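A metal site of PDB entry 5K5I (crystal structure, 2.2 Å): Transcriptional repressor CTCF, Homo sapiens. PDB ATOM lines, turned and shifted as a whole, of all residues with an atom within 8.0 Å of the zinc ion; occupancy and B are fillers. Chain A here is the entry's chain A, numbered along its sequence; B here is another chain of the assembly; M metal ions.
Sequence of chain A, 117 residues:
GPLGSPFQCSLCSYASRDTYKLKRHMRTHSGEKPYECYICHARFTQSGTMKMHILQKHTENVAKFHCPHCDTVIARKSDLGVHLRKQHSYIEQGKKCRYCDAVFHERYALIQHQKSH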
ATOM      1  N   GLU A  36      29.143 -31.692  13.656  1.00  0.00           N
ATOM      2  CA  GLU A  36      27.913 -31.613  12.878  1.00  0.00           C
ATOM      3  C   GLU A  36      27.527 -30.163  12.668  1.00  0.00           C
ATOM      4  O   GLU A  36      27.554 -29.363  13.615  1.00  0.00           O
ATOM      5  CB  GLU A  36      26.769 -32.368  13.586  1.00  0.00           C
ATOM      6  CG  GLU A  36      25.499 -32.460  12.772  1.00  0.00           C
ATOM      7  CD  GLU A  36      24.331 -32.993  13.581  1.00  0.00           C
ATOM      8  OE1 GLU A  36      24.328 -32.812  14.812  1.00  0.00           O
ATOM      9  OE2 GLU A  36      23.411 -33.595  12.969  1.00  0.00           O
ATOM     10  N   CYS A  37      27.169 -29.821  11.436  1.00  0.00           N
ATOM     11  CA  CYS A  37      26.683 -28.484  11.123  1.00  0.00           C
ATOM     12  C   CYS A  37      25.276 -28.305  11.676  1.00  0.00           C
ATOM     13  O   CYS A  37      24.378 -29.089  11.365  1.00  0.00           O
ATOM     14  CB  CYS A  37      26.699 -28.242   9.621  1.00  0.00           C
ATOM     15  SG  CYS A  37      25.944 -26.685   9.098  1.00  0.00           S
ATOM     16  N   TYR A  38      25.072 -27.266  12.482  1.00  0.00           N
ATOM     17  CA  TYR A  38      23.790 -27.081  13.147  1.00  0.00           C
ATOM     18  C   TYR A  38      22.675 -26.628  12.197  1.00  0.00           C
ATOM     19  O   TYR A  38      21.571 -26.363  12.691  1.00  0.00           O
ATOM     20  CB  TYR A  38      23.934 -26.071  14.291  1.00  0.00           C
ATOM     21  CG  TYR A  38      24.091 -24.638  13.841  1.00  0.00           C
ATOM     22  CD1 TYR A  38      25.317 -24.167  13.389  1.00  0.00           C
ATOM     23  CD2 TYR A  38      23.015 -23.759  13.868  1.00  0.00           C
ATOM     24  CE1 TYR A  38      25.457 -22.849  12.975  1.00  0.00           C
ATOM     25  CE2 TYR A  38      23.148 -22.452  13.460  1.00  0.00           C
ATOM     26  CZ  TYR A  38      24.374 -22.001  13.022  1.00  0.00           C
ATOM     27  OH  TYR A  38      24.516 -20.692  12.608  1.00  0.00           O
ATOM     28  N   ILE A  39      22.880 -26.550  10.885  1.00  0.00           N
ATOM     29  CA  ILE A  39      21.874 -26.067   9.949  1.00  0.00           C
ATOM     30  C   ILE A  39      21.370 -27.188   9.038  1.00  0.00           C
ATOM     31  O   ILE A  39      20.168 -27.374   8.882  1.00  0.00           O
ATOM     32  CB  ILE A  39      22.401 -24.879   9.121  1.00  0.00           C
ATOM     33  CG1 ILE A  39      22.759 -23.723  10.054  1.00  0.00           C
ATOM     34  CG2 ILE A  39      21.374 -24.433   8.098  1.00  0.00           C
ATOM     35  CD1 ILE A  39      23.233 -22.472   9.352  1.00  0.00           C
ATOM     36  N   CYS A  40      22.291 -27.937   8.433  1.00  0.00           N
ATOM     37  CA  CYS A  40      21.929 -29.062   7.581  1.00  0.00           C
ATOM     38  C   CYS A  40      22.313 -30.412   8.173  1.00  0.00           C
ATOM     39  O   CYS A  40      22.141 -31.436   7.512  1.00  0.00           O
ATOM     40  CB  CYS A  40      22.565 -28.906   6.186  1.00  0.00           C
ATOM     41  SG  CYS A  40      24.378 -28.804   6.176  1.00  0.00           S
ATOM     42  N   HIS A  41      22.837 -30.418   9.405  1.00  0.00           N
ATOM     43  CA  HIS A  41      23.234 -31.651  10.092  1.00  0.00           C
ATOM     44  C   HIS A  41      24.189 -32.480   9.245  1.00  0.00           C
ATOM     45  O   HIS A  41      24.095 -33.710   9.169  1.00  0.00           O
ATOM     46  CB  HIS A  41      22.014 -32.467  10.515  1.00  0.00           C
ATOM     47  CG  HIS A  41      21.004 -31.690  11.295  1.00  0.00           C
ATOM     48  ND1 HIS A  41      20.896 -31.779  12.668  1.00  0.00           N
ATOM     49  CD2 HIS A  41      20.065 -30.794  10.905  1.00  0.00           C
ATOM     50  CE1 HIS A  41      19.938 -30.970  13.090  1.00  0.00           C
ATOM     51  NE2 HIS A  41      19.416 -30.359  12.034  1.00  0.00           N
ATOM     52  N   ALA A  42      25.132 -31.802   8.593  1.00  0.00           N
ATOM     53  CA  ALA A  42      26.203 -32.455   7.854  1.00  0.00           C
ATOM     54  C   ALA A  42      27.365 -32.747   8.791  1.00  0.00           C
ATOM     55  O   ALA A  42      27.661 -31.959   9.691  1.00  0.00           O
ATOM     56  CB  ALA A  42      26.664 -31.583   6.687  1.00  0.00           C
ATOM     57  N   ARG A  43      28.034 -33.869   8.565  1.00  0.00           N
ATOM     58  CA  ARG A  43      29.071 -34.368   9.450  1.00  0.00           C
ATOM     59  C   ARG A  43      30.452 -34.177   8.842  1.00  0.00           C
ATOM     60  O   ARG A  43      30.618 -34.247   7.619  1.00  0.00           O
ATOM     61  CB  ARG A  43      28.842 -35.847   9.785  1.00  0.00           C
ATOM     62  CG  ARG A  43      27.480 -36.116  10.405  1.00  0.00           C
ATOM     63  CD  ARG A  43      27.213 -37.606  10.554  1.00  0.00           C
ATOM     64  NE  ARG A  43      25.879 -37.861  11.086  1.00  0.00           N
ATOM     65  CZ  ARG A  43      25.367 -39.071  11.282  1.00  0.00           C
ATOM     66  NH1 ARG A  43      26.084 -40.155  10.988  1.00  0.00           N
ATOM     67  NH2 ARG A  43      24.140 -39.205  11.771  1.00  0.00           N
ATOM     68  N   PHE A  44      31.434 -33.934   9.709  1.00  0.00           N
ATOM     69  CA  PHE A  44      32.800 -33.671   9.273  1.00  0.00           C
ATOM     70  C   PHE A  44      33.773 -34.312  10.248  1.00  0.00           C
ATOM     71  O   PHE A  44      33.449 -34.538  11.415  1.00  0.00           O
ATOM     72  CB  PHE A  44      33.066 -32.159   9.168  1.00  0.00           C
ATOM     73  CG  PHE A  44      32.023 -31.404   8.404  1.00  0.00           C
ATOM     74  CD1 PHE A  44      32.093 -31.312   7.029  1.00  0.00           C
ATOM     75  CD2 PHE A  44      30.960 -30.802   9.063  1.00  0.00           C
ATOM     76  CE1 PHE A  44      31.124 -30.623   6.312  1.00  0.00           C
ATOM     77  CE2 PHE A  44      29.996 -30.113   8.355  1.00  0.00           C
ATOM     78  CZ  PHE A  44      30.081 -30.027   6.984  1.00  0.00           C
ATOM     79  N   MET A  50      34.408 -27.939   9.335  1.00  0.00           N
ATOM     80  CA  MET A  50      33.012 -27.542   9.516  1.00  0.00           C
ATOM     81  C   MET A  50      32.858 -26.037   9.432  1.00  0.00           C
ATOM     82  O   MET A  50      31.876 -25.540   8.875  1.00  0.00           O
ATOM     83  CB  MET A  50      32.485 -28.067  10.849  1.00  0.00           C
ATOM     84  CG  MET A  50      31.022 -27.742  11.113  1.00  0.00           C
ATOM     85  SD  MET A  50      30.472 -28.253  12.748  1.00  0.00           S
ATOM     86  CE  MET A  50      31.510 -27.232  13.795  1.00  0.00           C
ATOM     87  N   HIS A  53      32.697 -25.029   5.959  1.00  0.00           N
ATOM     88  CA  HIS A  53      31.411 -25.393   5.375  1.00  0.00           C
ATOM     89  C   HIS A  53      30.348 -24.352   5.687  1.00  0.00           C
ATOM     90  O   HIS A  53      29.613 -23.909   4.799  1.00  0.00           O
ATOM     91  CB  HIS A  53      30.979 -26.774   5.872  1.00  0.00           C
ATOM     92  CG  HIS A  53      29.524 -27.069   5.655  1.00  0.00           C
ATOM     93  ND1 HIS A  53      29.046 -27.613   4.480  1.00  0.00           N
ATOM     94  CD2 HIS A  53      28.446 -26.884   6.447  1.00  0.00           C
ATOM     95  CE1 HIS A  53      27.735 -27.762   4.567  1.00  0.00           C
ATOM     96  NE2 HIS A  53      27.340 -27.329   5.747  1.00  0.00           N
ATOM     97  N   ILE A  54      30.240 -23.955   6.962  1.00  0.00           N
ATOM     98  CA  ILE A  54      29.233 -22.963   7.354  1.00  0.00           C
ATOM     99  C   ILE A  54      29.503 -21.637   6.667  1.00  0.00           C
ATOM    100  O   ILE A  54      28.573 -20.913   6.283  1.00  0.00           O
ATOM    101  CB  ILE A  54      29.216 -22.818   8.888  1.00  0.00           C
ATOM    102  CG1 ILE A  54      28.922 -24.170   9.545  1.00  0.00           C
ATOM    103  CG2 ILE A  54      28.177 -21.790   9.315  1.00  0.00           C
ATOM    104  CD1 ILE A  54      28.887 -24.130  11.057  1.00  0.00           C
ATOM    105  N   LEU A  55      30.778 -21.283   6.481  1.00  0.00           N
ATOM    106  CA  LEU A  55      31.117 -20.014   5.855  1.00  0.00           C
ATOM    107  C   LEU A  55      30.754 -20.005   4.379  1.00  0.00           C
ATOM    108  O   LEU A  55      30.184 -19.023   3.883  1.00  0.00           O
ATOM    109  CB  LEU A  55      32.609 -19.723   6.052  1.00  0.00           C
ATOM    110  CG  LEU A  55      33.139 -18.440   5.395  1.00  0.00           C
ATOM    111  CD1 LEU A  55      32.440 -17.223   5.974  1.00  0.00           C
ATOM    112  CD2 LEU A  55      34.645 -18.340   5.562  1.00  0.00           C
ATOM    113  N   LYS A  57      28.611 -21.848   2.565  1.00  0.00           N
ATOM    114  CA  LYS A  57      27.244 -22.152   2.159  1.00  0.00           C
ATOM    115  C   LYS A  57      26.204 -21.400   2.960  1.00  0.00           C
ATOM    116  O   LYS A  57      25.266 -20.825   2.379  1.00  0.00           O
ATOM    117  CB  LYS A  57      26.982 -23.663   2.251  1.00  0.00           C
ATOM    118  CG  LYS A  57      27.736 -24.483   1.228  1.00  0.00           C
ATOM    119  CD  LYS A  57      27.299 -25.937   1.262  1.00  0.00           C
ATOM    120  CE  LYS A  57      27.975 -26.753   0.167  1.00  0.00           C
ATOM    121  NZ  LYS A  57      27.504 -28.163   0.157  1.00  0.00           N
ATOM    122  N   HIS A  58      26.319 -21.378   4.283  1.00  0.00           N
ATOM    123  CA  HIS A  58      25.288 -20.827   5.140  1.00  0.00           C
ATOM    124  C   HIS A  58      25.527 -19.369   5.545  1.00  0.00           C
ATOM    125  O   HIS A  58      24.567 -18.694   5.926  1.00  0.00           O
ATOM    126  CB  HIS A  58      25.145 -21.678   6.412  1.00  0.00           C
ATOM    127  CG  HIS A  58      24.877 -23.128   6.139  1.00  0.00           C
ATOM    128  ND1 HIS A  58      24.155 -23.552   5.042  1.00  0.00           N
ATOM    129  CD2 HIS A  58      25.242 -24.245   6.805  1.00  0.00           C
ATOM    130  CE1 HIS A  58      24.085 -24.877   5.057  1.00  0.00           C
ATOM    131  NE2 HIS A  58      24.737 -25.321   6.121  1.00  0.00           N
ATOM    132  P    DA B   6      31.655 -29.386   2.366  1.00  0.00           P
ATOM    133  OP1  DA B   6      30.308 -29.469   2.964  1.00  0.00           O
ATOM    134  OP2  DA B   6      32.491 -28.188   2.612  1.00  0.00           O
ATOM    135  O5'  DA B   6      32.501 -30.674   2.802  1.00  0.00           O
ATOM    136  C5'  DA B   6      32.027 -31.970   2.465  1.00  0.00           C
ATOM    137  C4'  DA B   6      33.149 -33.001   2.570  1.00  0.00           C
ATOM    138  O4'  DA B   6      34.289 -32.554   1.788  1.00  0.00           O
ATOM    139  C3'  DA B   6      33.662 -33.249   3.990  1.00  0.00           C
ATOM    140  O3'  DA B   6      33.803 -34.652   4.219  1.00  0.00           O
ATOM    141  C2'  DA B   6      35.000 -32.512   4.020  1.00  0.00           C
ATOM    142  C1'  DA B   6      35.458 -32.593   2.573  1.00  0.00           C
ATOM    143  N9   DA B   6      36.315 -31.477   2.179  1.00  0.00           N
ATOM    144  C8   DA B   6      36.097 -30.149   2.433  1.00  0.00           C
ATOM    145  N7   DA B   6      37.038 -29.365   1.966  1.00  0.00           N
ATOM    146  C5   DA B   6      37.925 -30.232   1.349  1.00  0.00           C
ATOM    147  C6   DA B   6      39.123 -30.016   0.657  1.00  0.00           C
ATOM    148  N6   DA B   6      39.658 -28.813   0.460  1.00  0.00           N
ATOM    149  N1   DA B   6      39.771 -31.098   0.170  1.00  0.00           N
ATOM    150  C2   DA B   6      39.229 -32.313   0.372  1.00  0.00           C
ATOM    151  N3   DA B   6      38.104 -32.628   1.001  1.00  0.00           N
ATOM    152  C4   DA B   6      37.495 -31.540   1.476  1.00  0.00           C
HETATM  153 ZN    ZN M   1      25.638 -26.989   6.819  1.00  0.00          ZN
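N of Cys 37 is in hydrogen-bond range of O of Ala 42 (2.8 Å). A ring nitrogen (ND1) of His 53 is in hydrogen-bond range of OP1 of DA 6 of chain B, 2.7 Å away. The side-chain sulfur of Cys 37 sits close to the backbone NH of Ile 39, at 3.5 Å.
Four residues have an atom within 4 Å of the zinc ion: Cys 37, Cys 40, His 53 and His 58. The nearest printed residue that does not touch the zinc ion is Ile 39 (4.5 Å).
The zinc ion is bound by NE2 of His 58 (2.0 Å). The zinc ion is bound by a ring nitrogen (NE2) of His 53 (2.0 Å). SG of Cys 40 binds the zinc ion, at 2.3 Å. The zinc ion is bound by the side-chain sulfur (SG) of Cys 37 (2.3 Å). The zinc ion has four donor atoms within binding distance.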
